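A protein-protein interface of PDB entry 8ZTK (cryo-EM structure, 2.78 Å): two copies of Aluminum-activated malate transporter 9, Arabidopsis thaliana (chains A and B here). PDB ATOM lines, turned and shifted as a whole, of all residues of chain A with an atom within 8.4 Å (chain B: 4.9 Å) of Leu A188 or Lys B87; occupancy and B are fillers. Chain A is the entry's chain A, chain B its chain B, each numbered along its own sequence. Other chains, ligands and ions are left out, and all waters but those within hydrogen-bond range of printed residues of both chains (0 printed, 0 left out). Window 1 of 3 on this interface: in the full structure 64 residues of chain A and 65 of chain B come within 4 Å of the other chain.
NZ of Lys B87 lies within hydrogen-bond range of O of Leu A188 (2.8 Å).
O of Leu A188 sits at hydrogen-bond distance from NZ of Lys A193, 3.1 Å away.
NZ of Lys B87 is in hydrogen-bond range of SD of Met B80 (3.5 Å).
The side-chain hydroxyl of Ser B91 sits at hydrogen-bond distance from the backbone carbonyl oxygen of Lys B87 (2.7 Å).
CE2 of Phe A181 touches O of Ile B88, 3.8 Å away.
Ser B91 touches Phe A181 (CB to CD2, 3.7 Å).
CE2 of Phe B90 touches CG2 of Thr A184, at 3.9 Å.
C of Thr A184 touches OG of Ser B91, 3.8 Å away.
Phe A185 touches Met B80.
Phe A185 touches Ile B88.
Phe A185 touches Ser B91 (N to OG, 3.8 Å).
O of Leu A188 touches SD of Met B80, 3.9 Å away.
Of the printed residues of chain B, Thr A184 touches Phe B90 (3.9 Å) and Ser B91 (3.8 Å).
Of the printed residues of chain A, Met B80 touches Phe A185 and Leu A188.
Of the printed residues of chain A, Lys B87 touches Leu A188.
The nearest residue of chain A that does not touch Lys B87 is Lys A193 (4.02 Å).
Hydrophobic or aromatic side chains of chain B that line the printed part of chain A: Met B80, Ile B88 and Phe B90.
Of the 15 printed residues of chain A, 4 touch a printed residue of chain B.
Printed residues of chain A that touch a printed residue of chain B: Phe A181, Thr A184, Phe A185 and Leu A188.
No position is printed for both chains.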
ATOM      1  N   PHE A 181       1.800 -21.939 -15.336  1.00  0.00           N
ATOM      2  CA  PHE A 181       0.445 -21.408 -15.287  1.00  0.00           C
ATOM      3  C   PHE A 181       0.187 -20.699 -13.966  1.00  0.00           C
ATOM      4  O   PHE A 181      -0.363 -19.592 -13.951  1.00  0.00           O
ATOM      5  CB  PHE A 181      -0.577 -22.525 -15.508  1.00  0.00           C
ATOM      6  CG  PHE A 181      -2.006 -22.075 -15.364  1.00  0.00           C
ATOM      7  CD1 PHE A 181      -2.615 -22.030 -14.119  1.00  0.00           C
ATOM      8  CD2 PHE A 181      -2.738 -21.688 -16.472  1.00  0.00           C
ATOM      9  CE1 PHE A 181      -3.923 -21.609 -13.986  1.00  0.00           C
ATOM     10  CE2 PHE A 181      -4.048 -21.268 -16.344  1.00  0.00           C
ATOM     11  CZ  PHE A 181      -4.640 -21.229 -15.100  1.00  0.00           C
ATOM     12  N   LEU A 182       0.597 -21.299 -12.845  1.00  0.00           N
ATOM     13  CA  LEU A 182       0.289 -20.666 -11.568  1.00  0.00           C
ATOM     14  C   LEU A 182       1.134 -19.418 -11.351  1.00  0.00           C
ATOM     15  O   LEU A 182       0.636 -18.421 -10.805  1.00  0.00           O
ATOM     16  CB  LEU A 182       0.492 -21.656 -10.421  1.00  0.00           C
ATOM     17  CG  LEU A 182      -0.469 -22.845 -10.368  1.00  0.00           C
ATOM     18  CD1 LEU A 182       0.145 -24.004  -9.599  1.00  0.00           C
ATOM     19  CD2 LEU A 182      -1.797 -22.435  -9.754  1.00  0.00           C
ATOM     20  N   ALA A 183       2.375 -19.409 -11.853  1.00  0.00           N
ATOM     21  CA  ALA A 183       3.240 -18.255 -11.670  1.00  0.00           C
ATOM     22  C   ALA A 183       2.916 -17.139 -12.649  1.00  0.00           C
ATOM     23  O   ALA A 183       3.347 -16.002 -12.436  1.00  0.00           O
ATOM     24  CB  ALA A 183       4.707 -18.663 -11.813  1.00  0.00           C
ATOM     25  N   THR A 184       2.164 -17.435 -13.710  1.00  0.00           N
ATOM     26  CA  THR A 184       1.700 -16.380 -14.593  1.00  0.00           C
ATOM     27  C   THR A 184       0.315 -15.893 -14.203  1.00  0.00           C
ATOM     28  O   THR A 184      -0.051 -14.763 -14.547  1.00  0.00           O
ATOM     29  CB  THR A 184       1.684 -16.862 -16.045  1.00  0.00           C
ATOM     30  OG1 THR A 184       2.929 -17.503 -16.351  1.00  0.00           O
ATOM     31  CG2 THR A 184       1.480 -15.692 -16.992  1.00  0.00           C
ATOM     32  N   PHE A 185      -0.454 -16.716 -13.487  1.00  0.00           N
ATOM     33  CA  PHE A 185      -1.789 -16.332 -13.056  1.00  0.00           C
ATOM     34  C   PHE A 185      -1.790 -15.607 -11.719  1.00  0.00           C
ATOM     35  O   PHE A 185      -2.744 -14.877 -11.429  1.00  0.00           O
ATOM     36  CB  PHE A 185      -2.697 -17.561 -12.963  1.00  0.00           C
ATOM     37  CG  PHE A 185      -4.147 -17.224 -12.779  1.00  0.00           C
ATOM     38  CD1 PHE A 185      -4.930 -16.864 -13.861  1.00  0.00           C
ATOM     39  CD2 PHE A 185      -4.725 -17.261 -11.523  1.00  0.00           C
ATOM     40  CE1 PHE A 185      -6.263 -16.551 -13.694  1.00  0.00           C
ATOM     41  CE2 PHE A 185      -6.057 -16.948 -11.351  1.00  0.00           C
ATOM     42  CZ  PHE A 185      -6.827 -16.593 -12.437  1.00  0.00           C
ATOM     43  N   MET A 186      -0.751 -15.782 -10.901  1.00  0.00           N
ATOM     44  CA  MET A 186      -0.714 -15.110  -9.610  1.00  0.00           C
ATOM     45  C   MET A 186      -0.003 -13.766  -9.670  1.00  0.00           C
ATOM     46  O   MET A 186      -0.056 -13.009  -8.695  1.00  0.00           O
ATOM     47  CB  MET A 186      -0.038 -16.002  -8.565  1.00  0.00           C
ATOM     48  CG  MET A 186      -1.008 -16.800  -7.712  1.00  0.00           C
ATOM     49  SD  MET A 186      -0.213 -17.547  -6.278  1.00  0.00           S
ATOM     50  CE  MET A 186      -0.676 -19.263  -6.490  1.00  0.00           C
ATOM     51  N   LYS A 187       0.654 -13.456 -10.784  1.00  0.00           N
ATOM     52  CA  LYS A 187       1.279 -12.159 -11.002  1.00  0.00           C
ATOM     53  C   LYS A 187       0.314 -11.130 -11.581  1.00  0.00           C
ATOM     54  O   LYS A 187       0.673  -9.952 -11.680  1.00  0.00           O
ATOM     55  CB  LYS A 187       2.495 -12.319 -11.925  1.00  0.00           C
ATOM     56  CG  LYS A 187       3.101 -11.018 -12.416  1.00  0.00           C
ATOM     57  CD  LYS A 187       3.631 -11.145 -13.834  1.00  0.00           C
ATOM     58  CE  LYS A 187       2.658 -11.892 -14.730  1.00  0.00           C
ATOM     59  NZ  LYS A 187       3.331 -12.430 -15.942  1.00  0.00           N
ATOM     60  N   LEU A 188      -0.900 -11.540 -11.942  1.00  0.00           N
ATOM     61  CA  LEU A 188      -1.880 -10.676 -12.583  1.00  0.00           C
ATOM     62  C   LEU A 188      -2.978 -10.217 -11.632  1.00  0.00           C
ATOM     63  O   LEU A 188      -4.003  -9.701 -12.087  1.00  0.00           O
ATOM     64  CB  LEU A 188      -2.505 -11.383 -13.788  1.00  0.00           C
ATOM     65  CG  LEU A 188      -1.566 -11.864 -14.893  1.00  0.00           C
ATOM     66  CD1 LEU A 188      -2.255 -12.907 -15.755  1.00  0.00           C
ATOM     67  CD2 LEU A 188      -1.095 -10.694 -15.739  1.00  0.00           C
ATOM     68  N   TYR A 189      -2.792 -10.394 -10.335  1.00  0.00           N
ATOM     69  CA  TYR A 189      -3.795  -9.962  -9.369  1.00  0.00           C
ATOM     70  C   TYR A 189      -3.557  -8.504  -8.995  1.00  0.00           C
ATOM     71  O   TYR A 189      -2.413  -8.121  -8.727  1.00  0.00           O
ATOM     72  CB  TYR A 189      -3.739 -10.832  -8.121  1.00  0.00           C
ATOM     73  CG  TYR A 189      -5.091 -11.187  -7.551  1.00  0.00           C
ATOM     74  CD1 TYR A 189      -5.925 -10.211  -7.025  1.00  0.00           C
ATOM     75  CD2 TYR A 189      -5.536 -12.502  -7.542  1.00  0.00           C
ATOM     76  CE1 TYR A 189      -7.163 -10.533  -6.504  1.00  0.00           C
ATOM     77  CE2 TYR A 189      -6.771 -12.834  -7.022  1.00  0.00           C
ATOM     78  CZ  TYR A 189      -7.582 -11.846  -6.505  1.00  0.00           C
ATOM     79  OH  TYR A 189      -8.814 -12.172  -5.988  1.00  0.00           O
ATOM     80  N   PRO A 190      -4.600  -7.670  -8.966  1.00  0.00           N
ATOM     81  CA  PRO A 190      -4.378  -6.233  -8.733  1.00  0.00           C
ATOM     82  C   PRO A 190      -3.641  -5.926  -7.443  1.00  0.00           C
ATOM     83  O   PRO A 190      -2.951  -4.901  -7.367  1.00  0.00           O
ATOM     84  CB  PRO A 190      -5.804  -5.663  -8.721  1.00  0.00           C
ATOM     85  CG  PRO A 190      -6.595  -6.624  -9.542  1.00  0.00           C
ATOM     86  CD  PRO A 190      -6.015  -7.973  -9.238  1.00  0.00           C
ATOM     87  N   SER A 191      -3.765  -6.775  -6.423  1.00  0.00           N
ATOM     88  CA  SER A 191      -3.042  -6.539  -5.179  1.00  0.00           C
ATOM     89  C   SER A 191      -1.569  -6.906  -5.305  1.00  0.00           C
ATOM     90  O   SER A 191      -0.731  -6.352  -4.586  1.00  0.00           O
ATOM     91  CB  SER A 191      -3.686  -7.325  -4.036  1.00  0.00           C
ATOM     92  OG  SER A 191      -3.592  -8.720  -4.256  1.00  0.00           O
ATOM     93  N   MET A 192      -1.239  -7.829  -6.206  1.00  0.00           N
ATOM     94  CA  MET A 192       0.129  -8.295  -6.421  1.00  0.00           C
ATOM     95  C   MET A 192       0.733  -7.717  -7.694  1.00  0.00           C
ATOM     96  O   MET A 192       1.437  -8.416  -8.427  1.00  0.00           O
ATOM     97  CB  MET A 192       0.168  -9.819  -6.453  1.00  0.00           C
ATOM     98  CG  MET A 192       0.885 -10.449  -5.273  1.00  0.00           C
ATOM     99  SD  MET A 192      -0.199 -10.729  -3.861  1.00  0.00           S
ATOM    100  CE  MET A 192      -1.131 -12.147  -4.431  1.00  0.00           C
ATOM    101  N   LYS A 193       0.478  -6.441  -7.982  1.00  0.00           N
ATOM    102  CA  LYS A 193       0.942  -5.810  -9.210  1.00  0.00           C
ATOM    103  C   LYS A 193       2.181  -4.953  -8.991  1.00  0.00           C
ATOM    104  O   LYS A 193       2.517  -4.126  -9.847  1.00  0.00           O
ATOM    105  CB  LYS A 193      -0.174  -4.969  -9.832  1.00  0.00           C
ATOM    106  CG  LYS A 193      -1.480  -5.712 -10.036  1.00  0.00           C
ATOM    107  CD  LYS A 193      -1.398  -6.647 -11.230  1.00  0.00           C
ATOM    108  CE  LYS A 193      -2.766  -6.858 -11.859  1.00  0.00           C
ATOM    109  NZ  LYS A 193      -2.670  -7.218 -13.300  1.00  0.00           N
ATOM    110  N   GLU A 196       6.281  -8.154  -9.241  1.00  0.00           N
ATOM    111  CA  GLU A 196       6.437  -9.060 -10.373  1.00  0.00           C
ATOM    112  C   GLU A 196       7.840  -9.648 -10.437  1.00  0.00           C
ATOM    113  O   GLU A 196       8.039 -10.703 -11.057  1.00  0.00           O
ATOM    114  CB  GLU A 196       6.120  -8.332 -11.679  1.00  0.00           C
ATOM    115  CG  GLU A 196       4.640  -8.216 -11.986  1.00  0.00           C
ATOM    116  CD  GLU A 196       3.970  -7.101 -11.213  1.00  0.00           C
ATOM    117  OE1 GLU A 196       2.757  -7.212 -10.942  1.00  0.00           O
ATOM    118  OE2 GLU A 196       4.657  -6.114 -10.874  1.00  0.00           O
ATOM    119  N   PHE A 199       8.225 -12.994  -8.586  1.00  0.00           N
ATOM    120  CA  PHE A 199       7.609 -14.089  -9.324  1.00  0.00           C
ATOM    121  C   PHE A 199       8.432 -14.487 -10.544  1.00  0.00           C
ATOM    122  O   PHE A 199       8.540 -15.679 -10.864  1.00  0.00           O
ATOM    123  CB  PHE A 199       6.195 -13.697  -9.760  1.00  0.00           C
ATOM    124  CG  PHE A 199       5.173 -13.789  -8.664  1.00  0.00           C
ATOM    125  CD1 PHE A 199       4.796 -15.017  -8.150  1.00  0.00           C
ATOM    126  CD2 PHE A 199       4.589 -12.646  -8.150  1.00  0.00           C
ATOM    127  CE1 PHE A 199       3.857 -15.101  -7.142  1.00  0.00           C
ATOM    128  CE2 PHE A 199       3.651 -12.725  -7.142  1.00  0.00           C
ATOM    129  CZ  PHE A 199       3.283 -13.954  -6.638  1.00  0.00           C
ATOM    130  N   MET B  80     -11.756 -14.058 -10.236  1.00  0.00           N
ATOM    131  CA  MET B  80     -11.183 -13.287 -11.331  1.00  0.00           C
ATOM    132  C   MET B  80     -11.048 -14.130 -12.590  1.00  0.00           C
ATOM    133  O   MET B  80     -11.174 -13.607 -13.704  1.00  0.00           O
ATOM    134  CB  MET B  80      -9.825 -12.713 -10.923  1.00  0.00           C
ATOM    135  CG  MET B  80      -9.247 -11.723 -11.923  1.00  0.00           C
ATOM    136  SD  MET B  80      -7.472 -11.458 -11.735  1.00  0.00           S
ATOM    137  CE  MET B  80      -6.923 -13.105 -11.293  1.00  0.00           C
ATOM    138  N   ASP B  84     -12.798 -13.117 -15.799  1.00  0.00           N
ATOM    139  CA  ASP B  84     -11.853 -12.802 -16.871  1.00  0.00           C
ATOM    140  C   ASP B  84     -11.244 -14.082 -17.423  1.00  0.00           C
ATOM    141  O   ASP B  84     -10.262 -14.599 -16.860  1.00  0.00           O
ATOM    142  CB  ASP B  84     -10.760 -11.862 -16.367  1.00  0.00           C
ATOM    143  CG  ASP B  84     -10.496 -10.714 -17.319  1.00  0.00           C
ATOM    144  OD1 ASP B  84     -11.021 -10.748 -18.453  1.00  0.00           O
ATOM    145  OD2 ASP B  84      -9.766  -9.777 -16.935  1.00  0.00           O
ATOM    146  N   PRO B  85     -11.781 -14.633 -18.515  1.00  0.00           N
ATOM    147  CA  PRO B  85     -11.179 -15.832 -19.116  1.00  0.00           C
ATOM    148  C   PRO B  85      -9.941 -15.555 -19.957  1.00  0.00           C
ATOM    149  O   PRO B  85      -9.254 -16.509 -20.344  1.00  0.00           O
ATOM    150  CB  PRO B  85     -12.314 -16.392 -19.982  1.00  0.00           C
ATOM    151  CG  PRO B  85     -13.124 -15.195 -20.348  1.00  0.00           C
ATOM    152  CD  PRO B  85     -13.026 -14.230 -19.195  1.00  0.00           C
ATOM    153  N   ARG B  86      -9.639 -14.289 -20.252  1.00  0.00           N
ATOM    154  CA  ARG B  86      -8.444 -13.959 -21.024  1.00  0.00           C
ATOM    155  C   ARG B  86      -7.168 -14.244 -20.240  1.00  0.00           C
ATOM    156  O   ARG B  86      -6.174 -14.717 -20.806  1.00  0.00           O
ATOM    157  CB  ARG B  86      -8.494 -12.492 -21.446  1.00  0.00           C
ATOM    158  CG  ARG B  86      -9.688 -12.145 -22.317  1.00  0.00           C
ATOM    159  CD  ARG B  86      -9.377 -11.007 -23.273  1.00  0.00           C
ATOM    160  NE  ARG B  86      -8.648  -9.931 -22.615  1.00  0.00           N
ATOM    161  CZ  ARG B  86      -8.603  -8.680 -23.054  1.00  0.00           C
ATOM    162  NH1 ARG B  86      -9.234  -8.312 -24.156  1.00  0.00           N
ATOM    163  NH2 ARG B  86      -7.909  -7.776 -22.369  1.00  0.00           N
ATOM    164  N   LYS B  87      -7.174 -13.954 -18.938  1.00  0.00           N
ATOM    165  CA  LYS B  87      -6.001 -14.208 -18.108  1.00  0.00           C
ATOM    166  C   LYS B  87      -5.629 -15.688 -18.101  1.00  0.00           C
ATOM    167  O   LYS B  87      -4.442 -16.041 -18.158  1.00  0.00           O
ATOM    168  CB  LYS B  87      -6.273 -13.707 -16.692  1.00  0.00           C
ATOM    169  CG  LYS B  87      -6.424 -12.196 -16.606  1.00  0.00           C
ATOM    170  CD  LYS B  87      -5.887 -11.632 -15.304  1.00  0.00           C
ATOM    171  CE  LYS B  87      -5.695 -10.128 -15.406  1.00  0.00           C
ATOM    172  NZ  LYS B  87      -5.921  -9.442 -14.104  1.00  0.00           N
ATOM    173  N   ILE B  88      -6.630 -16.570 -18.074  1.00  0.00           N
ATOM    174  CA  ILE B  88      -6.351 -18.002 -18.075  1.00  0.00           C
ATOM    175  C   ILE B  88      -5.753 -18.425 -19.410  1.00  0.00           C
ATOM    176  O   ILE B  88      -4.848 -19.268 -19.465  1.00  0.00           O
ATOM    177  CB  ILE B  88      -7.632 -18.793 -17.757  1.00  0.00           C
ATOM    178  CG1 ILE B  88      -8.092 -18.517 -16.326  1.00  0.00           C
ATOM    179  CG2 ILE B  88      -7.409 -20.282 -17.969  1.00  0.00           C
ATOM    180  CD1 ILE B  88      -9.474 -19.044 -16.025  1.00  0.00           C
ATOM    181  N   VAL B  89      -6.213 -17.814 -20.502  1.00  0.00           N
ATOM    182  CA  VAL B  89      -5.664 -18.131 -21.815  1.00  0.00           C
ATOM    183  C   VAL B  89      -4.207 -17.696 -21.897  1.00  0.00           C
ATOM    184  O   VAL B  89      -3.347 -18.444 -22.370  1.00  0.00           O
ATOM    185  CB  VAL B  89      -6.514 -17.482 -22.922  1.00  0.00           C
ATOM    186  CG1 VAL B  89      -5.837 -17.644 -24.273  1.00  0.00           C
ATOM    187  CG2 VAL B  89      -7.906 -18.088 -22.943  1.00  0.00           C
ATOM    188  N   PHE B  90      -3.914 -16.471 -21.458  1.00  0.00           N
ATOM    189  CA  PHE B  90      -2.535 -15.990 -21.468  1.00  0.00           C
ATOM    190  C   PHE B  90      -1.623 -16.890 -20.636  1.00  0.00           C
ATOM    191  O   PHE B  90      -0.511 -17.241 -21.068  1.00  0.00           O
ATOM    192  CB  PHE B  90      -2.502 -14.548 -20.955  1.00  0.00           C
ATOM    193  CG  PHE B  90      -1.133 -13.933 -20.933  1.00  0.00           C
ATOM    194  CD1 PHE B  90      -0.439 -13.714 -22.110  1.00  0.00           C
ATOM    195  CD2 PHE B  90      -0.551 -13.552 -19.736  1.00  0.00           C
ATOM    196  CE1 PHE B  90       0.816 -13.140 -22.090  1.00  0.00           C
ATOM    197  CE2 PHE B  90       0.703 -12.978 -19.711  1.00  0.00           C
ATOM    198  CZ  PHE B  90       1.387 -12.772 -20.889  1.00  0.00           C
ATOM    199  N   SER B  91      -2.086 -17.297 -19.449  1.00  0.00           N
ATOM    200  CA  SER B  91      -1.245 -18.122 -18.587  1.00  0.00           C
ATOM    201  C   SER B  91      -1.040 -19.521 -19.155  1.00  0.00           C
ATOM    202  O   SER B  91       0.063 -20.077 -19.050  1.00  0.00           O
ATOM    203  CB  SER B  91      -1.857 -18.196 -17.191  1.00  0.00           C
ATOM    204  OG  SER B  91      -2.292 -16.917 -16.768  1.00  0.00           O
